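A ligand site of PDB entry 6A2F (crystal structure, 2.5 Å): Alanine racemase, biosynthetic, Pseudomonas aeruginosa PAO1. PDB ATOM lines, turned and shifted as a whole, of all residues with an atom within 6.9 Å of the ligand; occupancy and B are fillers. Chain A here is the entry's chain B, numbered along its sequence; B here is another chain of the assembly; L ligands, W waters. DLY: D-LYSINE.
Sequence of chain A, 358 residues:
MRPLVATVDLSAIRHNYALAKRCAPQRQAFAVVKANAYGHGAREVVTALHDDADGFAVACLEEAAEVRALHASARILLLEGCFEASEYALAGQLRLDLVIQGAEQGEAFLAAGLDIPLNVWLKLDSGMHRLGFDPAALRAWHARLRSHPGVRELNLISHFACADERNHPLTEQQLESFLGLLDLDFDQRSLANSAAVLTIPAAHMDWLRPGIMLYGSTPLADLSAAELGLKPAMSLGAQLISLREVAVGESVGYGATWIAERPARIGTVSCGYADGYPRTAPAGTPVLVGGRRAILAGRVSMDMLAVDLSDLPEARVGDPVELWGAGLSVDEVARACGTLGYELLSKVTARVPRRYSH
OP2 of LLP 34 of chain B sits at hydrogen-bond distance from the side-chain hydroxyl (OH) of Tyr 342 of chain B. The side-chain hydroxyl (OH) of Tyr 254 sits at hydrogen-bond distance from a ring nitrogen (NE2) of His 159 of chain B (2.7 Å). NH1 of Arg 130 of chain B is in hydrogen-bond range of OG of Ser 301, 2.6 Å away. N1 of LLP 34 of chain B sits at hydrogen-bond distance from a ring nitrogen (ND1) of His 159 of chain B (3.2 Å). OH of Tyr 38 of chain B lies within hydrogen-bond range of OP1 of LLP 34 of chain B (2.7 Å). The backbone NH of Tyr 273 lies within hydrogen-bond range of the backbone carbonyl oxygen of Met 302 (3.2 Å). N of Tyr 273 lies within hydrogen-bond range of O of Ser 301.
Tyr 254 touches the ligand (OH to CG, 3.4 Å). Tyr 342 of chain B touches the ligand. Hydrophobic or aromatic side chains within 4 Å of the ligand: Tyr 254, Tyr 273, Met 302, Met 304 and Tyr 342 of chain B. Nine residues have an atom within 4 Å of the ligand: Tyr 254, Tyr 273, Ser 301, Met 302, Asp 303, Met 304, LLP 34 of chain B, Arg 130 of chain B and Tyr 342 of chain B. The nearest printed residue that does not touch the ligand is Glu 80 of chain B (4.3 Å).
Water W1 bridges OE2 of Glu 80 of chain B and OXT of the ligand.
An oxygen (O) of the ligand is in hydrogen-bond range of the backbone NH (N) of Met 302. O3 of LLP 34 of chain B sits at hydrogen-bond distance from an oxygen (OXT) of the ligand (3.3 Å). The backbone NH (N) of Asp 303 sits at hydrogen-bond distance from an oxygen (O) of the ligand (2.8 Å). The side-chain hydroxyl (OG) of Ser 301 sits at hydrogen-bond distance from a nitrogen (N) of the ligand (3.1 Å). The side-chain carboxylate of Asp 303 sits close to an oxygen (OXT) of the ligand (2.8 Å). OH of Tyr 273 lies within hydrogen-bond range of NZ of the ligand (2.7 Å). An oxygen (O) of the ligand lies within hydrogen-bond range of the backbone NH (N) of Met 304. N of the ligand lies close to NH1 of Arg 130 of chain B.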
ATOM      1  N   TYR A 254     -17.357 -10.245 -22.685  1.00  0.00           N
ATOM      2  CA  TYR A 254     -18.706  -9.780 -22.359  1.00  0.00           C
ATOM      3  C   TYR A 254     -19.594  -9.618 -23.582  1.00  0.00           C
ATOM      4  O   TYR A 254     -19.141  -9.168 -24.641  1.00  0.00           O
ATOM      5  CB  TYR A 254     -18.636  -8.456 -21.604  1.00  0.00           C
ATOM      6  CG  TYR A 254     -18.195  -8.567 -20.169  1.00  0.00           C
ATOM      7  CD1 TYR A 254     -18.910  -9.350 -19.264  1.00  0.00           C
ATOM      8  CD2 TYR A 254     -17.077  -7.878 -19.710  1.00  0.00           C
ATOM      9  CE1 TYR A 254     -18.509  -9.442 -17.934  1.00  0.00           C
ATOM     10  CE2 TYR A 254     -16.664  -7.967 -18.387  1.00  0.00           C
ATOM     11  CZ  TYR A 254     -17.381  -8.756 -17.504  1.00  0.00           C
ATOM     12  OH  TYR A 254     -16.999  -8.866 -16.185  1.00  0.00           O
ATOM     13  N   GLY A 272      -6.901  -2.687 -18.696  1.00  0.00           N
ATOM     14  CA  GLY A 272      -8.340  -2.501 -18.900  1.00  0.00           C
ATOM     15  C   GLY A 272      -8.725  -1.036 -18.839  1.00  0.00           C
ATOM     16  O   GLY A 272      -7.843  -0.177 -18.797  1.00  0.00           O
ATOM     17  N   TYR A 273     -10.025  -0.739 -18.829  1.00  0.00           N
ATOM     18  CA  TYR A 273     -10.471   0.652 -18.832  1.00  0.00           C
ATOM     19  C   TYR A 273     -10.171   1.409 -17.541  1.00  0.00           C
ATOM     20  O   TYR A 273     -10.001   2.636 -17.581  1.00  0.00           O
ATOM     21  CB  TYR A 273     -11.940   0.832 -19.294  1.00  0.00           C
ATOM     22  CG  TYR A 273     -12.991   0.063 -18.535  1.00  0.00           C
ATOM     23  CD1 TYR A 273     -13.477   0.515 -17.303  1.00  0.00           C
ATOM     24  CD2 TYR A 273     -13.542  -1.102 -19.065  1.00  0.00           C
ATOM     25  CE1 TYR A 273     -14.449  -0.192 -16.615  1.00  0.00           C
ATOM     26  CE2 TYR A 273     -14.519  -1.809 -18.385  1.00  0.00           C
ATOM     27  CZ  TYR A 273     -14.965  -1.348 -17.165  1.00  0.00           C
ATOM     28  OH  TYR A 273     -15.927  -2.058 -16.505  1.00  0.00           O
ATOM     29  N   ARG A 279     -13.061   1.625 -22.936  1.00  0.00           N
ATOM     30  CA  ARG A 279     -13.873   0.420 -22.732  1.00  0.00           C
ATOM     31  C   ARG A 279     -14.414  -0.116 -24.050  1.00  0.00           C
ATOM     32  O   ARG A 279     -14.444  -1.337 -24.272  1.00  0.00           O
ATOM     33  CB  ARG A 279     -15.028   0.688 -21.769  1.00  0.00           C
ATOM     34  CG  ARG A 279     -15.841  -0.557 -21.482  1.00  0.00           C
ATOM     35  CD  ARG A 279     -17.076  -0.299 -20.634  1.00  0.00           C
ATOM     36  NE  ARG A 279     -18.039  -1.374 -20.859  1.00  0.00           N
ATOM     37  CZ  ARG A 279     -18.972  -1.372 -21.806  1.00  0.00           C
ATOM     38  NH1 ARG A 279     -19.110  -0.324 -22.627  1.00  0.00           N
ATOM     39  NH2 ARG A 279     -19.787  -2.401 -21.944  1.00  0.00           N
ATOM     40  N   VAL A 300     -13.241  -4.893 -23.901  1.00  0.00           N
ATOM     41  CA  VAL A 300     -12.254  -4.489 -22.916  1.00  0.00           C
ATOM     42  C   VAL A 300     -12.930  -4.480 -21.540  1.00  0.00           C
ATOM     43  O   VAL A 300     -14.001  -3.901 -21.364  1.00  0.00           O
ATOM     44  CB  VAL A 300     -11.653  -3.095 -23.253  1.00  0.00           C
ATOM     45  CG1 VAL A 300     -10.719  -2.599 -22.164  1.00  0.00           C
ATOM     46  CG2 VAL A 300     -10.923  -3.132 -24.589  1.00  0.00           C
ATOM     47  N   SER A 301     -12.298  -5.163 -20.580  1.00  0.00           N
ATOM     48  CA  SER A 301     -12.763  -5.185 -19.194  1.00  0.00           C
ATOM     49  C   SER A 301     -12.129  -4.055 -18.376  1.00  0.00           C
ATOM     50  O   SER A 301     -11.286  -3.305 -18.880  1.00  0.00           O
ATOM     51  CB  SER A 301     -12.391  -6.516 -18.556  1.00  0.00           C
ATOM     52  OG  SER A 301     -13.412  -7.460 -18.744  1.00  0.00           O
ATOM     53  N   MET A 302     -12.526  -3.963 -17.103  1.00  0.00           N
ATOM     54  CA  MET A 302     -11.944  -2.994 -16.178  1.00  0.00           C
ATOM     55  C   MET A 302     -10.437  -3.172 -16.012  1.00  0.00           C
ATOM     56  O   MET A 302      -9.694  -2.183 -15.958  1.00  0.00           O
ATOM     57  CB  MET A 302     -12.647  -3.084 -14.815  1.00  0.00           C
ATOM     58  CG  MET A 302     -12.351  -1.919 -13.890  1.00  0.00           C
ATOM     59  SD  MET A 302     -13.343  -1.878 -12.385  1.00  0.00           S
ATOM     60  CE  MET A 302     -14.954  -1.476 -13.079  1.00  0.00           C
ATOM     61  N   ASP A 303      -9.985  -4.422 -15.940  1.00  0.00           N
ATOM     62  CA  ASP A 303      -8.593  -4.724 -15.634  1.00  0.00           C
ATOM     63  C   ASP A 303      -7.896  -5.561 -16.709  1.00  0.00           C
ATOM     64  O   ASP A 303      -6.683  -5.748 -16.654  1.00  0.00           O
ATOM     65  CB  ASP A 303      -8.503  -5.428 -14.278  1.00  0.00           C
ATOM     66  CG  ASP A 303      -9.179  -4.653 -13.176  1.00  0.00           C
ATOM     67  OD1 ASP A 303      -8.685  -3.556 -12.817  1.00  0.00           O
ATOM     68  OD2 ASP A 303     -10.221  -5.119 -12.658  1.00  0.00           O
ATOM     69  N   MET A 304      -8.683  -6.080 -17.638  1.00  0.00           N
ATOM     70  CA  MET A 304      -8.159  -6.968 -18.660  1.00  0.00           C
ATOM     71  C   MET A 304      -8.592  -6.661 -20.076  1.00  0.00           C
ATOM     72  O   MET A 304      -9.622  -6.059 -20.327  1.00  0.00           O
ATOM     73  CB  MET A 304      -8.489  -8.416 -18.322  1.00  0.00           C
ATOM     74  CG  MET A 304      -7.873  -8.896 -17.033  1.00  0.00           C
ATOM     75  SD  MET A 304      -8.472 -10.520 -16.568  1.00  0.00           S
ATOM     76  CE  MET A 304     -10.080 -10.124 -15.910  1.00  0.00           C
ATOM     77  N   LEU A 305      -7.757  -7.066 -21.014  1.00  0.00           N
ATOM     78  CA  LEU A 305      -7.992  -6.886 -22.441  1.00  0.00           C
ATOM     79  C   LEU A 305      -7.668  -8.191 -23.166  1.00  0.00           C
ATOM     80  O   LEU A 305      -6.878  -8.997 -22.689  1.00  0.00           O
ATOM     81  CB  LEU A 305      -7.127  -5.739 -22.981  1.00  0.00           C
ATOM     82  CG  LEU A 305      -6.785  -5.787 -24.477  1.00  0.00           C
ATOM     83  CD1 LEU A 305      -6.083  -4.506 -24.899  1.00  0.00           C
ATOM     84  CD2 LEU A 305      -5.935  -7.008 -24.802  1.00  0.00           C
ATOM     85  N1  LLP B  34     -16.330 -11.163 -10.367  1.00  0.00           N
ATOM     86  C2  LLP B  34     -15.102 -10.969 -10.916  1.00  0.00           C
ATOM     87  C2' LLP B  34     -14.216 -12.157 -11.194  1.00  0.00           C
ATOM     88  C3  LLP B  34     -14.642  -9.590 -11.243  1.00  0.00           C
ATOM     89  O3  LLP B  34     -13.410  -9.359 -11.785  1.00  0.00           O
ATOM     90  C4  LLP B  34     -15.561  -8.460 -10.944  1.00  0.00           C
ATOM     91  C4' LLP B  34     -15.218  -7.012 -11.231  1.00  0.00           C
ATOM     92  C5  LLP B  34     -16.874  -8.818 -10.349  1.00  0.00           C
ATOM     93  C6  LLP B  34     -17.185 -10.164 -10.096  1.00  0.00           C
ATOM     94  C5' LLP B  34     -17.879  -7.742 -10.033  1.00  0.00           C
ATOM     95  OP4 LLP B  34     -18.520  -7.408 -11.265  1.00  0.00           O
ATOM     96  P   LLP B  34     -19.801  -6.419 -11.306  1.00  0.00           P
ATOM     97  OP1 LLP B  34     -19.214  -5.045 -11.038  1.00  0.00           O
ATOM     98  OP2 LLP B  34     -20.374  -6.567 -12.698  1.00  0.00           O
ATOM     99  OP3 LLP B  34     -20.696  -6.958 -10.212  1.00  0.00           O
ATOM    100  N   LLP B  34     -12.093  -3.332  -6.276  1.00  0.00           N
ATOM    101  CA  LLP B  34     -10.957  -3.137  -7.187  1.00  0.00           C
ATOM    102  CB  LLP B  34     -10.887  -4.291  -8.180  1.00  0.00           C
ATOM    103  CG  LLP B  34     -11.906  -4.202  -9.313  1.00  0.00           C
ATOM    104  CD  LLP B  34     -12.294  -5.597  -9.795  1.00  0.00           C
ATOM    105  CE  LLP B  34     -13.257  -5.495 -10.971  1.00  0.00           C
ATOM    106  NZ  LLP B  34     -13.795  -6.796 -11.329  1.00  0.00           N
ATOM    107  C   LLP B  34     -11.040  -1.808  -7.918  1.00  0.00           C
ATOM    108  O   LLP B  34     -12.101  -1.166  -7.946  1.00  0.00           O
ATOM    109  N   TYR B  38     -13.845   1.243  -7.777  1.00  0.00           N
ATOM    110  CA  TYR B  38     -14.527   1.762  -8.963  1.00  0.00           C
ATOM    111  C   TYR B  38     -14.486   3.293  -8.960  1.00  0.00           C
ATOM    112  O   TYR B  38     -15.486   3.955  -9.266  1.00  0.00           O
ATOM    113  CB  TYR B  38     -15.971   1.247  -9.020  1.00  0.00           C
ATOM    114  CG  TYR B  38     -16.150  -0.231  -9.316  1.00  0.00           C
ATOM    115  CD1 TYR B  38     -15.395  -1.220  -8.670  1.00  0.00           C
ATOM    116  CD2 TYR B  38     -17.116  -0.657 -10.230  1.00  0.00           C
ATOM    117  CE1 TYR B  38     -15.573  -2.569  -8.940  1.00  0.00           C
ATOM    118  CE2 TYR B  38     -17.318  -2.004 -10.498  1.00  0.00           C
ATOM    119  CZ  TYR B  38     -16.552  -2.954  -9.861  1.00  0.00           C
ATOM    120  OH  TYR B  38     -16.762  -4.288 -10.137  1.00  0.00           O
ATOM    121  N   ALA B  59      -8.344  -6.734  -7.693  1.00  0.00           N
ATOM    122  CA  ALA B  59      -7.788  -7.184  -8.976  1.00  0.00           C
ATOM    123  C   ALA B  59      -6.282  -7.549  -8.960  1.00  0.00           C
ATOM    124  O   ALA B  59      -5.787  -8.217  -9.886  1.00  0.00           O
ATOM    125  CB  ALA B  59      -8.070  -6.136 -10.050  1.00  0.00           C
ATOM    126  N   LEU B  79      -8.731 -11.698  -7.440  1.00  0.00           N
ATOM    127  CA  LEU B  79      -9.591 -12.217  -8.511  1.00  0.00           C
ATOM    128  C   LEU B  79      -8.817 -12.860  -9.665  1.00  0.00           C
ATOM    129  O   LEU B  79      -9.269 -13.836 -10.250  1.00  0.00           O
ATOM    130  CB  LEU B  79     -10.520 -11.124  -9.042  1.00  0.00           C
ATOM    131  CG  LEU B  79     -11.617 -10.636  -8.078  1.00  0.00           C
ATOM    132  CD1 LEU B  79     -12.197  -9.304  -8.543  1.00  0.00           C
ATOM    133  CD2 LEU B  79     -12.707 -11.671  -7.901  1.00  0.00           C
ATOM    134  N   GLU B  80      -7.655 -12.294  -9.992  1.00  0.00           N
ATOM    135  CA  GLU B  80      -6.825 -12.801 -11.081  1.00  0.00           C
ATOM    136  C   GLU B  80      -5.646 -13.618 -10.568  1.00  0.00           C
ATOM    137  O   GLU B  80      -4.811 -14.067 -11.365  1.00  0.00           O
ATOM    138  CB  GLU B  80      -6.318 -11.636 -11.949  1.00  0.00           C
ATOM    139  CG  GLU B  80      -7.419 -10.844 -12.641  1.00  0.00           C
ATOM    140  CD  GLU B  80      -6.893  -9.551 -13.263  1.00  0.00           C
ATOM    141  OE1 GLU B  80      -5.774  -9.579 -13.830  1.00  0.00           O
ATOM    142  OE2 GLU B  80      -7.606  -8.526 -13.199  1.00  0.00           O
ATOM    143  N   MET B 128     -16.673 -17.332 -20.991  1.00  0.00           N
ATOM    144  CA  MET B 128     -16.075 -15.999 -21.140  1.00  0.00           C
ATOM    145  C   MET B 128     -14.898 -16.067 -22.115  1.00  0.00           C
ATOM    146  O   MET B 128     -14.659 -15.155 -22.899  1.00  0.00           O
ATOM    147  CB  MET B 128     -15.597 -15.456 -19.798  1.00  0.00           C
ATOM    148  CG  MET B 128     -16.514 -14.422 -19.173  1.00  0.00           C
ATOM    149  SD  MET B 128     -16.302 -12.777 -19.869  1.00  0.00           S
ATOM    150  CE  MET B 128     -16.485 -11.793 -18.402  1.00  0.00           C
ATOM    151  N   ARG B 130     -11.551 -16.021 -21.592  1.00  0.00           N
ATOM    152  CA  ARG B 130     -10.304 -15.279 -21.381  1.00  0.00           C
ATOM    153  C   ARG B 130      -9.452 -15.946 -20.305  1.00  0.00           C
ATOM    154  O   ARG B 130      -8.363 -16.457 -20.597  1.00  0.00           O
ATOM    155  CB  ARG B 130     -10.569 -13.802 -21.078  1.00  0.00           C
ATOM    156  CG  ARG B 130     -11.040 -12.995 -22.273  1.00  0.00           C
ATOM    157  CD  ARG B 130     -11.118 -11.504 -21.972  1.00  0.00           C
ATOM    158  NE  ARG B 130     -11.813 -11.239 -20.715  1.00  0.00           N
ATOM    159  CZ  ARG B 130     -12.007 -10.043 -20.183  1.00  0.00           C
ATOM    160  NH1 ARG B 130     -12.638  -9.934 -19.022  1.00  0.00           N
ATOM    161  NH2 ARG B 130     -11.556  -8.946 -20.798  1.00  0.00           N
ATOM    162  N   LEU B 131      -9.963 -15.975 -19.076  1.00  0.00           N
ATOM    163  CA  LEU B 131      -9.276 -16.606 -17.955  1.00  0.00           C
ATOM    164  C   LEU B 131      -9.963 -17.898 -17.541  1.00  0.00           C
ATOM    165  O   LEU B 131     -11.166 -18.055 -17.731  1.00  0.00           O
ATOM    166  CB  LEU B 131      -9.211 -15.645 -16.762  1.00  0.00           C
ATOM    167  CG  LEU B 131      -8.458 -14.318 -16.917  1.00  0.00           C
ATOM    168  CD1 LEU B 131      -8.617 -13.529 -15.646  1.00  0.00           C
ATOM    169  CD2 LEU B 131      -6.977 -14.518 -17.241  1.00  0.00           C
ATOM    170  N   HIS B 159     -17.237 -16.852 -13.923  1.00  0.00           N
ATOM    171  CA  HIS B 159     -17.784 -15.519 -14.141  1.00  0.00           C
ATOM    172  C   HIS B 159     -18.611 -15.478 -15.437  1.00  0.00           C
ATOM    173  O   HIS B 159     -18.162 -15.969 -16.474  1.00  0.00           O
ATOM    174  CB  HIS B 159     -16.640 -14.502 -14.187  1.00  0.00           C
ATOM    175  CG  HIS B 159     -17.087 -13.067 -14.204  1.00  0.00           C
ATOM    176  ND1 HIS B 159     -17.546 -12.417 -13.079  1.00  0.00           N
ATOM    177  CD2 HIS B 159     -17.120 -12.154 -15.203  1.00  0.00           C
ATOM    178  CE1 HIS B 159     -17.854 -11.169 -13.392  1.00  0.00           C
ATOM    179  NE2 HIS B 159     -17.609 -10.987 -14.676  1.00  0.00           N
ATOM    180  N   LEU B 340     -20.900   2.160 -20.508  1.00  0.00           N
ATOM    181  CA  LEU B 340     -21.593   1.833 -19.253  1.00  0.00           C
ATOM    182  C   LEU B 340     -21.063   2.611 -18.045  1.00  0.00           C
ATOM    183  O   LEU B 340     -19.953   3.158 -18.079  1.00  0.00           O
ATOM    184  CB  LEU B 340     -21.517   0.331 -18.967  1.00  0.00           C
ATOM    185  CG  LEU B 340     -22.147  -0.682 -19.921  1.00  0.00           C
ATOM    186  CD1 LEU B 340     -21.767  -2.082 -19.455  1.00  0.00           C
ATOM    187  CD2 LEU B 340     -23.660  -0.525 -19.990  1.00  0.00           C
ATOM    188  N   TYR B 342     -19.794   1.650 -15.315  1.00  0.00           N
ATOM    189  CA  TYR B 342     -18.468   1.165 -14.950  1.00  0.00           C
ATOM    190  C   TYR B 342     -17.370   2.143 -15.369  1.00  0.00           C
ATOM    191  O   TYR B 342     -16.554   2.543 -14.552  1.00  0.00           O
ATOM    192  CB  TYR B 342     -18.177  -0.177 -15.631  1.00  0.00           C
ATOM    193  CG  TYR B 342     -19.037  -1.371 -15.275  1.00  0.00           C
ATOM    194  CD1 TYR B 342     -18.774  -2.116 -14.128  1.00  0.00           C
ATOM    195  CD2 TYR B 342     -20.066  -1.783 -16.121  1.00  0.00           C
ATOM    196  CE1 TYR B 342     -19.541  -3.237 -13.829  1.00  0.00           C
ATOM    197  CE2 TYR B 342     -20.837  -2.891 -15.820  1.00  0.00           C
ATOM    198  CZ  TYR B 342     -20.576  -3.622 -14.673  1.00  0.00           C
ATOM    199  OH  TYR B 342     -21.342  -4.722 -14.375  1.00  0.00           O
HETATM  200  N   DLY L   1     -13.504  -9.008 -16.044  1.00  0.00           N
HETATM  201  CA  DLY L   1     -13.515  -7.878 -15.060  1.00  0.00           C
HETATM  202  C   DLY L   1     -12.130  -7.335 -14.788  1.00  0.00           C
HETATM  203  O   DLY L   1     -11.407  -6.877 -15.678  1.00  0.00           O
HETATM  204  CB  DLY L   1     -14.408  -6.757 -15.589  1.00  0.00           C
HETATM  205  CG  DLY L   1     -15.462  -6.343 -14.565  1.00  0.00           C
HETATM  206  CD  DLY L   1     -16.071  -4.987 -14.911  1.00  0.00           C
HETATM  207  CE  DLY L   1     -17.096  -5.110 -16.040  1.00  0.00           C
HETATM  208  NZ  DLY L   1     -16.473  -4.632 -17.254  1.00  0.00           N
HETATM  209  OXT DLY L   1     -11.672  -7.312 -13.646  1.00  0.00           O
HETATM  210  O   HOH W   1      -9.969  -8.602 -11.930  1.00  0.00           O
